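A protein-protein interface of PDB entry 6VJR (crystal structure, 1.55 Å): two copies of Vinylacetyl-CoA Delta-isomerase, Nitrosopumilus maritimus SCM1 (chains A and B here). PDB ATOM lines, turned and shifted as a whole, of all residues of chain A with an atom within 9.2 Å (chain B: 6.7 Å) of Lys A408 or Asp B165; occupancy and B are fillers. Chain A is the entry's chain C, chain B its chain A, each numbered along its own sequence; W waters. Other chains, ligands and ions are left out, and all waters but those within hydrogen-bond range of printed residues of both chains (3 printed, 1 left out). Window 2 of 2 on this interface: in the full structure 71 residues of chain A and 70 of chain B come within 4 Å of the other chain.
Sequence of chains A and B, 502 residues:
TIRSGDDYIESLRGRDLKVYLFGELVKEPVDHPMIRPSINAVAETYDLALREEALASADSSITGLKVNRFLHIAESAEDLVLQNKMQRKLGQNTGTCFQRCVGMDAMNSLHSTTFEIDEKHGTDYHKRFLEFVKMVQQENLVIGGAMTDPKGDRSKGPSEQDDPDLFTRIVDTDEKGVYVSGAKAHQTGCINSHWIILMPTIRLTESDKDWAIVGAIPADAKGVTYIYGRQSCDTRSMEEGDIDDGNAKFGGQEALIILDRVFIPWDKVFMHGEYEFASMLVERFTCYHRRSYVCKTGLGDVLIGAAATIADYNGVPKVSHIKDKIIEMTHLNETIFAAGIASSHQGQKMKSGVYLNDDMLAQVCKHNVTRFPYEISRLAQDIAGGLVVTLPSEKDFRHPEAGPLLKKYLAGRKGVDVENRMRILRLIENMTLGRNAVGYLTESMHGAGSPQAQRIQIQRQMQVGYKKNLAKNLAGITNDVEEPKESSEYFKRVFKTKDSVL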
ATOM      1  N   PHE A 397     -21.851 -23.944  12.905  1.00  0.00           N
ATOM      2  CA  PHE A 397     -20.514 -23.830  12.356  1.00  0.00           C
ATOM      3  C   PHE A 397     -19.851 -25.212  12.188  1.00  0.00           C
ATOM      4  O   PHE A 397     -18.993 -25.390  11.336  1.00  0.00           O
ATOM      5  CB  PHE A 397     -19.663 -22.960  13.282  1.00  0.00           C
ATOM      6  CG  PHE A 397     -18.289 -22.661  12.728  1.00  0.00           C
ATOM      7  CD1 PHE A 397     -18.154 -21.901  11.563  1.00  0.00           C
ATOM      8  CD2 PHE A 397     -17.152 -23.057  13.418  1.00  0.00           C
ATOM      9  CE1 PHE A 397     -16.895 -21.624  11.049  1.00  0.00           C
ATOM     10  CE2 PHE A 397     -15.883 -22.809  12.892  1.00  0.00           C
ATOM     11  CZ  PHE A 397     -15.760 -22.064  11.727  1.00  0.00           C
ATOM     12  N   GLU A 401     -22.828 -29.396   6.486  1.00  0.00           N
ATOM     13  CA  GLU A 401     -23.362 -28.615   5.396  1.00  0.00           C
ATOM     14  C   GLU A 401     -23.421 -27.124   5.723  1.00  0.00           C
ATOM     15  O   GLU A 401     -22.986 -26.287   4.920  1.00  0.00           O
ATOM     16  CB  GLU A 401     -24.746 -29.157   5.046  1.00  0.00           C
ATOM     17  CG  GLU A 401     -24.674 -30.592   4.528  1.00  0.00           C
ATOM     18  CD  GLU A 401     -26.039 -31.181   4.344  1.00  0.00           C
ATOM     19  OE1 GLU A 401     -26.534 -30.920   3.196  1.00  0.00           O
ATOM     20  OE2 GLU A 401     -26.582 -31.811   5.324  1.00  0.00           O
ATOM     21  N   ALA A 402     -23.984 -26.772   6.887  1.00  0.00           N
ATOM     22  CA  ALA A 402     -24.050 -25.368   7.282  1.00  0.00           C
ATOM     23  C   ALA A 402     -22.661 -24.784   7.575  1.00  0.00           C
ATOM     24  O   ALA A 402     -22.429 -23.604   7.300  1.00  0.00           O
ATOM     25  CB  ALA A 402     -24.975 -25.159   8.473  1.00  0.00           C
ATOM     26  N   GLY A 403     -21.760 -25.622   8.098  1.00  0.00           N
ATOM     27  CA  GLY A 403     -20.451 -25.158   8.510  1.00  0.00           C
ATOM     28  C   GLY A 403     -19.647 -24.597   7.347  1.00  0.00           C
ATOM     29  O   GLY A 403     -19.093 -23.488   7.430  1.00  0.00           O
ATOM     30  N   PRO A 404     -19.489 -25.357   6.228  1.00  0.00           N
ATOM     31  CA  PRO A 404     -18.788 -24.798   5.087  1.00  0.00           C
ATOM     32  C   PRO A 404     -19.350 -23.486   4.570  1.00  0.00           C
ATOM     33  O   PRO A 404     -18.594 -22.645   4.101  1.00  0.00           O
ATOM     34  CB  PRO A 404     -18.771 -25.916   4.060  1.00  0.00           C
ATOM     35  CG  PRO A 404     -18.820 -27.146   4.955  1.00  0.00           C
ATOM     36  CD  PRO A 404     -19.733 -26.804   6.074  1.00  0.00           C
ATOM     37  N   LEU A 405     -20.676 -23.361   4.605  1.00  0.00           N
ATOM     38  CA  LEU A 405     -21.341 -22.144   4.165  1.00  0.00           C
ATOM     39  C   LEU A 405     -20.939 -20.973   5.067  1.00  0.00           C
ATOM     40  O   LEU A 405     -20.737 -19.869   4.599  1.00  0.00           O
ATOM     41  CB  LEU A 405     -22.849 -22.339   4.179  1.00  0.00           C
ATOM     42  CG  LEU A 405     -23.358 -23.379   3.177  1.00  0.00           C
ATOM     43  CD1 LEU A 405     -24.860 -23.525   3.343  1.00  0.00           C
ATOM     44  CD2 LEU A 405     -22.990 -23.042   1.764  1.00  0.00           C
ATOM     45  N   LEU A 406     -20.864 -21.213   6.385  1.00  0.00           N
ATOM     46  CA  LEU A 406     -20.463 -20.180   7.340  1.00  0.00           C
ATOM     47  C   LEU A 406     -18.999 -19.789   7.148  1.00  0.00           C
ATOM     48  O   LEU A 406     -18.675 -18.597   7.163  1.00  0.00           O
ATOM     49  CB  LEU A 406     -20.777 -20.601   8.761  1.00  0.00           C
ATOM     50  CG  LEU A 406     -22.265 -20.747   9.067  1.00  0.00           C
ATOM     51  CD1 LEU A 406     -22.547 -21.388  10.377  1.00  0.00           C
ATOM     52  CD2 LEU A 406     -22.997 -19.423   8.994  1.00  0.00           C
ATOM     53  N   LYS A 407     -18.130 -20.780   6.928  1.00  0.00           N
ATOM     54  CA  LYS A 407     -16.717 -20.521   6.691  1.00  0.00           C
ATOM     55  C   LYS A 407     -16.545 -19.644   5.460  1.00  0.00           C
ATOM     56  O   LYS A 407     -15.748 -18.709   5.460  1.00  0.00           O
ATOM     57  CB  LYS A 407     -15.922 -21.824   6.615  1.00  0.00           C
ATOM     58  CG  LYS A 407     -15.769 -22.477   7.972  1.00  0.00           C
ATOM     59  CD  LYS A 407     -15.100 -23.845   7.958  1.00  0.00           C
ATOM     60  CE  LYS A 407     -15.054 -24.462   9.305  1.00  0.00           C
ATOM     61  NZ  LYS A 407     -16.325 -24.892   9.899  1.00  0.00           N
ATOM     62  N   LYS A 408     -17.346 -19.904   4.432  1.00  0.00           N
ATOM     63  CA  LYS A 408     -17.262 -19.112   3.219  1.00  0.00           C
ATOM     64  C   LYS A 408     -17.804 -17.697   3.444  1.00  0.00           C
ATOM     65  O   LYS A 408     -17.166 -16.711   3.096  1.00  0.00           O
ATOM     66  CB  LYS A 408     -18.123 -19.764   2.124  1.00  0.00           C
ATOM     67  CG  LYS A 408     -18.232 -19.050   0.834  1.00  0.00           C
ATOM     68  CD  LYS A 408     -19.078 -19.838  -0.169  1.00  0.00           C
ATOM     69  CE  LYS A 408     -19.459 -19.109  -1.430  1.00  0.00           C
ATOM     70  NZ  LYS A 408     -18.366 -18.786  -2.335  1.00  0.00           N
ATOM     71  N   TYR A 409     -19.038 -17.609   3.961  1.00  0.00           N
ATOM     72  CA  TYR A 409     -19.780 -16.365   3.902  1.00  0.00           C
ATOM     73  C   TYR A 409     -19.461 -15.401   5.048  1.00  0.00           C
ATOM     74  O   TYR A 409     -19.736 -14.199   4.900  1.00  0.00           O
ATOM     75  CB  TYR A 409     -21.288 -16.613   3.819  1.00  0.00           C
ATOM     76  CG  TYR A 409     -21.671 -16.952   2.388  1.00  0.00           C
ATOM     77  CD1 TYR A 409     -21.564 -15.963   1.418  1.00  0.00           C
ATOM     78  CD2 TYR A 409     -22.086 -18.215   1.992  1.00  0.00           C
ATOM     79  CE1 TYR A 409     -21.924 -16.193   0.105  1.00  0.00           C
ATOM     80  CE2 TYR A 409     -22.411 -18.476   0.663  1.00  0.00           C
ATOM     81  CZ  TYR A 409     -22.301 -17.466  -0.280  1.00  0.00           C
ATOM     82  OH  TYR A 409     -22.601 -17.671  -1.581  1.00  0.00           O
ATOM     83  N   LEU A 410     -18.889 -15.895   6.164  1.00  0.00           N
ATOM     84  CA  LEU A 410     -18.576 -15.030   7.291  1.00  0.00           C
ATOM     85  C   LEU A 410     -17.112 -14.607   7.274  1.00  0.00           C
ATOM     86  O   LEU A 410     -16.541 -14.199   8.294  1.00  0.00           O
ATOM     87  CB  LEU A 410     -19.006 -15.622   8.633  1.00  0.00           C
ATOM     88  CG  LEU A 410     -20.504 -15.922   8.708  1.00  0.00           C
ATOM     89  CD1 LEU A 410     -20.818 -16.352  10.124  1.00  0.00           C
ATOM     90  CD2 LEU A 410     -21.343 -14.744   8.301  1.00  0.00           C
ATOM     91  N   ALA A 411     -16.494 -14.698   6.098  1.00  0.00           N
ATOM     92  CA  ALA A 411     -15.147 -14.192   5.909  1.00  0.00           C
ATOM     93  C   ALA A 411     -15.060 -12.711   6.276  1.00  0.00           C
ATOM     94  O   ALA A 411     -16.000 -11.941   6.042  1.00  0.00           O
ATOM     95  CB  ALA A 411     -14.738 -14.398   4.460  1.00  0.00           C
ATOM     96  N   GLY A 412     -13.918 -12.327   6.874  1.00  0.00           N
ATOM     97  CA  GLY A 412     -13.558 -10.920   6.943  1.00  0.00           C
ATOM     98  C   GLY A 412     -12.501 -10.606   5.890  1.00  0.00           C
ATOM     99  O   GLY A 412     -12.568 -11.075   4.757  1.00  0.00           O
ATOM    100  N   VAL A 416      -7.893 -13.926   7.545  1.00  0.00           N
ATOM    101  CA  VAL A 416      -8.508 -14.062   8.847  1.00  0.00           C
ATOM    102  C   VAL A 416      -9.254 -15.381   8.912  1.00  0.00           C
ATOM    103  O   VAL A 416     -10.108 -15.654   8.057  1.00  0.00           O
ATOM    104  CB  VAL A 416      -9.458 -12.886   9.133  1.00  0.00           C
ATOM    105  CG1 VAL A 416     -10.268 -13.142  10.376  1.00  0.00           C
ATOM    106  CG2 VAL A 416      -8.669 -11.605   9.264  1.00  0.00           C
ATOM    107  N   VAL A 418     -12.125 -17.596  10.007  1.00  0.00           N
ATOM    108  CA  VAL A 418     -13.494 -17.300  10.377  1.00  0.00           C
ATOM    109  C   VAL A 418     -13.798 -17.696  11.817  1.00  0.00           C
ATOM    110  O   VAL A 418     -14.499 -16.961  12.516  1.00  0.00           O
ATOM    111  CB  VAL A 418     -14.506 -17.903   9.394  1.00  0.00           C
ATOM    112  CG1 VAL A 418     -15.943 -17.825   9.908  1.00  0.00           C
ATOM    113  CG2 VAL A 418     -14.414 -17.164   8.082  1.00  0.00           C
ATOM    114  N   GLU A 419     -13.200 -18.787  12.310  1.00  0.00           N
ATOM    115  CA  GLU A 419     -13.479 -19.151  13.688  1.00  0.00           C
ATOM    116  C   GLU A 419     -12.975 -18.060  14.655  1.00  0.00           C
ATOM    117  O   GLU A 419     -13.594 -17.830  15.694  1.00  0.00           O
ATOM    118  CB  GLU A 419     -12.835 -20.486  14.028  1.00  0.00           C
ATOM    119  CG  GLU A 419     -13.098 -20.948  15.457  1.00  0.00           C
ATOM    120  CD  GLU A 419     -12.589 -22.335  15.800  1.00  0.00           C
ATOM    121  OE1 GLU A 419     -12.436 -23.173  14.877  1.00  0.00           O
ATOM    122  OE2 GLU A 419     -12.285 -22.561  17.011  1.00  0.00           O
ATOM    123  N   ARG A 421     -12.893 -14.828  14.010  1.00  0.00           N
ATOM    124  CA  ARG A 421     -13.837 -13.730  13.918  1.00  0.00           C
ATOM    125  C   ARG A 421     -15.101 -14.062  14.726  1.00  0.00           C
ATOM    126  O   ARG A 421     -15.619 -13.224  15.456  1.00  0.00           O
ATOM    127  CB  ARG A 421     -14.125 -13.473  12.439  1.00  0.00           C
ATOM    128  CG  ARG A 421     -15.002 -12.266  12.179  1.00  0.00           C
ATOM    129  CD  ARG A 421     -14.954 -11.799  10.716  1.00  0.00           C
ATOM    130  NE  ARG A 421     -15.763 -10.620  10.453  1.00  0.00           N
ATOM    131  CZ  ARG A 421     -17.016 -10.642   9.909  1.00  0.00           C
ATOM    132  NH1 ARG A 421     -17.561 -11.750   9.394  1.00  0.00           N
ATOM    133  NH2 ARG A 421     -17.735  -9.536   9.849  1.00  0.00           N
ATOM    134  N   MET A 422     -15.565 -15.319  14.636  1.00  0.00           N
ATOM    135  CA  MET A 422     -16.687 -15.778  15.455  1.00  0.00           C
ATOM    136  C   MET A 422     -16.398 -15.641  16.953  1.00  0.00           C
ATOM    137  O   MET A 422     -17.212 -15.144  17.750  1.00  0.00           O
ATOM    138  CB  MET A 422     -17.086 -17.198  15.069  1.00  0.00           C
ATOM    139  CG  MET A 422     -17.690 -17.247  13.694  1.00  0.00           C
ATOM    140  SD  MET A 422     -18.190 -18.907  13.226  1.00  0.00           S
ATOM    141  CE  MET A 422     -19.886 -19.008  13.822  1.00  0.00           C
ATOM    142  N   ASP B 149     -25.617  -7.831   2.476  1.00  0.00           N
ATOM    143  CA  ASP B 149     -24.798  -8.998   2.204  1.00  0.00           C
ATOM    144  C   ASP B 149     -23.790  -9.151   3.347  1.00  0.00           C
ATOM    145  O   ASP B 149     -23.641  -8.283   4.215  1.00  0.00           O
ATOM    146  CB  ASP B 149     -24.026  -8.850   0.897  1.00  0.00           C
ATOM    147  CG  ASP B 149     -24.923  -8.419  -0.256  1.00  0.00           C
ATOM    148  OD1 ASP B 149     -25.185  -7.202  -0.328  1.00  0.00           O
ATOM    149  OD2 ASP B 149     -25.446  -9.297  -0.966  1.00  0.00           O
ATOM    150  N   PRO B 150     -23.098 -10.301   3.432  1.00  0.00           N
ATOM    151  CA  PRO B 150     -22.064 -10.474   4.445  1.00  0.00           C
ATOM    152  C   PRO B 150     -20.904  -9.485   4.338  1.00  0.00           C
ATOM    153  O   PRO B 150     -20.384  -9.116   5.384  1.00  0.00           O
ATOM    154  CB  PRO B 150     -21.638 -11.924   4.280  1.00  0.00           C
ATOM    155  CG  PRO B 150     -22.833 -12.587   3.639  1.00  0.00           C
ATOM    156  CD  PRO B 150     -23.350 -11.534   2.709  1.00  0.00           C
ATOM    157  N   PRO B 158     -17.670  -4.924  -4.119  1.00  0.00           N
ATOM    158  CA  PRO B 158     -17.970  -6.271  -4.580  1.00  0.00           C
ATOM    159  C   PRO B 158     -16.951  -6.868  -5.533  1.00  0.00           C
ATOM    160  O   PRO B 158     -16.536  -8.011  -5.355  1.00  0.00           O
ATOM    161  CB  PRO B 158     -19.314  -6.120  -5.285  1.00  0.00           C
ATOM    162  CG  PRO B 158     -19.930  -4.956  -4.524  1.00  0.00           C
ATOM    163  CD  PRO B 158     -18.802  -3.999  -4.272  1.00  0.00           C
ATOM    164  N   GLN B 161     -13.581  -8.088  -3.793  1.00  0.00           N
ATOM    165  CA  GLN B 161     -13.510  -9.174  -2.829  1.00  0.00           C
ATOM    166  C   GLN B 161     -12.795 -10.376  -3.457  1.00  0.00           C
ATOM    167  O   GLN B 161     -12.900 -10.662  -4.670  1.00  0.00           O
ATOM    168  CB  GLN B 161     -14.904  -9.606  -2.372  1.00  0.00           C
ATOM    169  CG  GLN B 161     -15.723  -8.500  -1.718  1.00  0.00           C
ATOM    170  CD  GLN B 161     -15.147  -8.058  -0.393  1.00  0.00           C
ATOM    171  OE1 GLN B 161     -14.599  -8.877   0.370  1.00  0.00           O
ATOM    172  NE2 GLN B 161     -15.329  -6.781  -0.106  1.00  0.00           N
ATOM    173  N   ASP B 162     -12.094 -11.114  -2.602  1.00  0.00           N
ATOM    174  CA  ASP B 162     -11.404 -12.338  -2.976  1.00  0.00           C
ATOM    175  C   ASP B 162     -12.413 -13.402  -3.425  1.00  0.00           C
ATOM    176  O   ASP B 162     -12.102 -14.221  -4.264  1.00  0.00           O
ATOM    177  CB  ASP B 162     -10.629 -12.843  -1.767  1.00  0.00           C
ATOM    178  CG  ASP B 162      -9.479 -13.806  -2.024  1.00  0.00           C
ATOM    179  OD1 ASP B 162      -8.603 -13.453  -2.831  1.00  0.00           O
ATOM    180  OD2 ASP B 162      -9.434 -14.869  -1.347  1.00  0.00           O
ATOM    181  N   ASP B 163     -13.570 -13.447  -2.765  1.00  0.00           N
ATOM    182  CA  ASP B 163     -14.658 -14.350  -3.115  1.00  0.00           C
ATOM    183  C   ASP B 163     -15.796 -13.500  -3.645  1.00  0.00           C
ATOM    184  O   ASP B 163     -16.395 -12.730  -2.923  1.00  0.00           O
ATOM    185  CB  ASP B 163     -15.096 -15.174  -1.914  1.00  0.00           C
ATOM    186  CG  ASP B 163     -16.246 -16.140  -2.150  1.00  0.00           C
ATOM    187  OD1 ASP B 163     -16.833 -16.133  -3.284  1.00  0.00           O
ATOM    188  OD2 ASP B 163     -16.594 -16.863  -1.178  1.00  0.00           O
ATOM    189  N   PRO B 164     -16.118 -13.586  -4.945  1.00  0.00           N
ATOM    190  CA  PRO B 164     -17.142 -12.725  -5.509  1.00  0.00           C
ATOM    191  C   PRO B 164     -18.540 -12.914  -4.920  1.00  0.00           C
ATOM    192  O   PRO B 164     -19.349 -12.038  -5.092  1.00  0.00           O
ATOM    193  CB  PRO B 164     -17.072 -13.012  -6.999  1.00  0.00           C
ATOM    194  CG  PRO B 164     -16.622 -14.446  -6.989  1.00  0.00           C
ATOM    195  CD  PRO B 164     -15.537 -14.493  -5.956  1.00  0.00           C
ATOM    196  N   ASP B 165     -18.817 -14.047  -4.261  1.00  0.00           N
ATOM    197  CA  ASP B 165     -20.125 -14.342  -3.700  1.00  0.00           C
ATOM    198  C   ASP B 165     -20.391 -13.577  -2.401  1.00  0.00           C
ATOM    199  O   ASP B 165     -21.482 -13.671  -1.863  1.00  0.00           O
ATOM    200  CB  ASP B 165     -20.275 -15.830  -3.443  1.00  0.00           C
ATOM    201  CG  ASP B 165     -20.245 -16.696  -4.692  1.00  0.00           C
ATOM    202  OD1 ASP B 165     -20.603 -16.177  -5.778  1.00  0.00           O
ATOM    203  OD2 ASP B 165     -19.835 -17.873  -4.570  1.00  0.00           O
ATOM    204  N   LEU B 166     -19.411 -12.809  -1.865  1.00  0.00           N
ATOM    205  CA  LEU B 166     -19.595 -12.137  -0.585  1.00  0.00           C
ATOM    206  C   LEU B 166     -20.575 -10.966  -0.665  1.00  0.00           C
ATOM    207  O   LEU B 166     -21.053 -10.461   0.366  1.00  0.00           O
ATOM    208  CB  LEU B 166     -18.268 -11.729   0.033  1.00  0.00           C
ATOM    209  CG  LEU B 166     -17.384 -12.883   0.508  1.00  0.00           C
ATOM    210  CD1 LEU B 166     -15.931 -12.513   0.814  1.00  0.00           C
ATOM    211  CD2 LEU B 166     -18.007 -13.474   1.746  1.00  0.00           C
ATOM    212  N   PHE B 167     -20.886 -10.559  -1.902  1.00  0.00           N
ATOM    213  CA  PHE B 167     -22.068  -9.783  -2.215  1.00  0.00           C
ATOM    214  C   PHE B 167     -22.848 -10.581  -3.254  1.00  0.00           C
ATOM    215  O   PHE B 167     -22.248 -11.202  -4.147  1.00  0.00           O
ATOM    216  CB  PHE B 167     -21.714  -8.408  -2.798  1.00  0.00           C
ATOM    217  CG  PHE B 167     -21.067  -7.413  -1.854  1.00  0.00           C
ATOM    218  CD1 PHE B 167     -19.724  -7.545  -1.507  1.00  0.00           C
ATOM    219  CD2 PHE B 167     -21.772  -6.337  -1.361  1.00  0.00           C
ATOM    220  CE1 PHE B 167     -19.117  -6.613  -0.698  1.00  0.00           C
ATOM    221  CE2 PHE B 167     -21.161  -5.421  -0.511  1.00  0.00           C
ATOM    222  CZ  PHE B 167     -19.825  -5.548  -0.220  1.00  0.00           C
ATOM    223  N   THR B 168     -24.172 -10.507  -3.181  1.00  0.00           N
ATOM    224  CA  THR B 168     -25.064 -11.269  -4.041  1.00  0.00           C
ATOM    225  C   THR B 168     -24.991 -10.798  -5.500  1.00  0.00           C
ATOM    226  O   THR B 168     -25.039  -9.606  -5.804  1.00  0.00           O
ATOM    227  CB  THR B 168     -26.479 -11.171  -3.464  1.00  0.00           C
ATOM    228  OG1 THR B 168     -26.502 -11.779  -2.178  1.00  0.00           O
ATOM    229  CG2 THR B 168     -27.505 -11.887  -4.323  1.00  0.00           C
ATOM    230  N   ARG B 169     -24.867 -11.762  -6.410  1.00  0.00           N
ATOM    231  CA  ARG B 169     -24.655 -11.456  -7.818  1.00  0.00           C
ATOM    232  C   ARG B 169     -25.404 -12.410  -8.751  1.00  0.00           C
ATOM    233  O   ARG B 169     -25.781 -13.520  -8.389  1.00  0.00           O
ATOM    234  CB  ARG B 169     -23.167 -11.539  -8.150  1.00  0.00           C
ATOM    235  CG  ARG B 169     -22.613 -12.945  -7.941  1.00  0.00           C
ATOM    236  CD  ARG B 169     -21.105 -12.965  -8.056  1.00  0.00           C
ATOM    237  NE  ARG B 169     -20.510 -14.291  -7.826  1.00  0.00           N
ATOM    238  CZ  ARG B 169     -19.952 -15.045  -8.763  1.00  0.00           C
ATOM    239  NH1 ARG B 169     -19.667 -14.508  -9.906  1.00  0.00           N
ATOM    240  NH2 ARG B 169     -19.555 -16.278  -8.520  1.00  0.00           N
ATOM    241  N   VAL B 171     -25.139 -14.983 -11.564  1.00  0.00           N
ATOM    242  CA  VAL B 171     -24.141 -15.935 -12.034  1.00  0.00           C
ATOM    243  C   VAL B 171     -24.489 -16.534 -13.393  1.00  0.00           C
ATOM    244  O   VAL B 171     -23.603 -17.105 -14.033  1.00  0.00           O
ATOM    245  CB  VAL B 171     -23.880 -17.032 -10.995  1.00  0.00           C
ATOM    246  CG1 VAL B 171     -23.252 -16.473  -9.724  1.00  0.00           C
ATOM    247  CG2 VAL B 171     -25.097 -17.845 -10.633  1.00  0.00           C
ATOM    248  N   SER B 181     -26.386 -16.068  -6.875  1.00  0.00           N
ATOM    249  CA  SER B 181     -25.680 -16.689  -5.775  1.00  0.00           C
ATOM    250  C   SER B 181     -25.136 -15.596  -4.859  1.00  0.00           C
ATOM    251  O   SER B 181     -24.819 -14.483  -5.295  1.00  0.00           O
ATOM    252  CB  SER B 181     -24.554 -17.589  -6.269  1.00  0.00           C
ATOM    253  OG  SER B 181     -25.054 -18.677  -7.034  1.00  0.00           O
ATOM    254  N   GLY B 182     -24.996 -15.960  -3.582  1.00  0.00           N
ATOM    255  CA  GLY B 182     -24.490 -15.054  -2.578  1.00  0.00           C
ATOM    256  C   GLY B 182     -25.230 -15.332  -1.279  1.00  0.00           C
ATOM    257  O   GLY B 182     -25.625 -16.460  -1.010  1.00  0.00           O
ATOM    258  N   ALA B 183     -25.342 -14.314  -0.446  1.00  0.00           N
ATOM    259  CA  ALA B 183     -26.025 -14.465   0.822  1.00  0.00           C
ATOM    260  C   ALA B 183     -26.523 -13.102   1.275  1.00  0.00           C
ATOM    261  O   ALA B 183     -25.984 -12.075   0.827  1.00  0.00           O
ATOM    262  CB  ALA B 183     -25.084 -15.044   1.823  1.00  0.00           C
ATOM    263  N   TRP B 211     -23.552  -7.382  -9.809  1.00  0.00           N
ATOM    264  CA  TRP B 211     -24.167  -7.276  -8.503  1.00  0.00           C
ATOM    265  C   TRP B 211     -25.367  -6.328  -8.514  1.00  0.00           C
ATOM    266  O   TRP B 211     -26.026  -6.181  -7.497  1.00  0.00           O
ATOM    267  CB  TRP B 211     -23.113  -6.833  -7.471  1.00  0.00           C
ATOM    268  CG  TRP B 211     -22.059  -7.864  -7.181  1.00  0.00           C
ATOM    269  CD1 TRP B 211     -22.077  -8.752  -6.159  1.00  0.00           C
ATOM    270  CD2 TRP B 211     -20.821  -8.110  -7.901  1.00  0.00           C
ATOM    271  NE1 TRP B 211     -20.958  -9.540  -6.181  1.00  0.00           N
ATOM    272  CE2 TRP B 211     -20.158  -9.164  -7.216  1.00  0.00           C
ATOM    273  CE3 TRP B 211     -20.204  -7.551  -9.025  1.00  0.00           C
ATOM    274  CZ2 TRP B 211     -18.924  -9.658  -7.617  1.00  0.00           C
ATOM    275  CZ3 TRP B 211     -18.967  -8.026  -9.411  1.00  0.00           C
ATOM    276  CH2 TRP B 211     -18.349  -9.075  -8.728  1.00  0.00           C
ATOM    277  N   LEU B 259     -27.858 -18.215  -0.899  1.00  0.00           N
ATOM    278  CA  LEU B 259     -28.417 -18.393  -2.234  1.00  0.00           C
ATOM    279  C   LEU B 259     -27.436 -19.146  -3.127  1.00  0.00           C
ATOM    280  O   LEU B 259     -26.292 -18.691  -3.319  1.00  0.00           O
ATOM    281  CB  LEU B 259     -28.673 -17.007  -2.825  1.00  0.00           C
ATOM    282  CG  LEU B 259     -29.467 -16.038  -1.940  1.00  0.00           C
ATOM    283  CD1 LEU B 259     -29.310 -14.587  -2.363  1.00  0.00           C
ATOM    284  CD2 LEU B 259     -30.907 -16.408  -1.923  1.00  0.00           C
HETATM  285  O   HOH W   1     -19.688 -11.138   7.796  1.00  0.00           O
HETATM  286  O   HOH W   2     -15.292 -16.615   1.208  1.00  0.00           O
HETATM  287  O   HOH W   3     -23.895 -19.802  -2.592  1.00  0.00           O
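Pro A404 touches none of the printed residues of chain B. Lys A408 touches three residues of chain B. Printed residues of chain B within 4 Å of Tyr A409: Pro B150, Asp B165, Leu B166, Gly B182 and Ala B183. Printed residues of chain A within 4 Å of Asp B163: Lys A408 (2.9 Å). Leu B166 touches just these residues of chain A: Lys A408 (3.6 Å) and Tyr A409 (3.7 Å). Of the printed residues of chain A, Ala B183 touches Tyr A409. The nearest residue of chain B that does not touch Lys A408 is Pro B164 (6.2 Å). The nearest printed residue of chain B that does not touch Tyr A409 is Leu B259 (4.2 Å).
Water W2 bridges the backbone carbonyl oxygen (O) of Lys A408 (2.7 Å) and the side-chain carboxylate (OD2) of Asp B163 (2.7 Å). Water W3 lies within hydrogen-bond range of the side-chain hydroxyl of Tyr A409 and the backbone carbonyl oxygen of Leu B259. Water W1 bridges NH1 of Arg A421 and O of Pro B150.
The backbone carbonyl oxygen of Gly B182 is in hydrogen-bond range of the backbone NH of Leu B259. The backbone NH (N) of Asp B165 lies within hydrogen-bond range of the side-chain carboxylate (OD1) of Asp B163 (3.0 Å). OG1 of Thr B168 sits at hydrogen-bond distance from O of Ala B183, at 3.1 Å. OD1 of Asp B165 is in salt-bridge range of NE of Arg B169 (2.8 Å).
The side-chain amino group of Lys A408 lies within salt-bridge range of the side-chain carboxylate of Asp B163, at 2.9 Å. OH of Tyr A409 lies within hydrogen-bond range of O of Gly B182 (3.3 Å). NZ of Lys A408 is in salt-bridge range of OD2 of Asp B165, at 2.8 Å.
Of the 18 printed residues of chain B, 6 touch a printed residue of chain A. Hydrophobic or aromatic side chains of chain B within 4 Å of the printed part of chain A: Pro B150, Leu B166 and Ala B183. Hydrophobic or aromatic side chains of chain A that line the printed part of chain B: Tyr A409. Along chain A the printed residues that touch a printed residue of chain B span positions 408 to 409.
Leu B166 touches Lys A408 (CD2 to O, 3.6 Å). Tyr A409 touches Pro B150. O of Asp B165 touches CE1 of Tyr A409, 3.2 Å away. CD2 of Leu B166 touches O of Tyr A409, 3.7 Å away. Ala B183 touches Tyr A409.
No position is printed for both chains. Of the 8 pairs that touch across the chains among the printed residues, none has its exchanged pair printed and touching as well.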
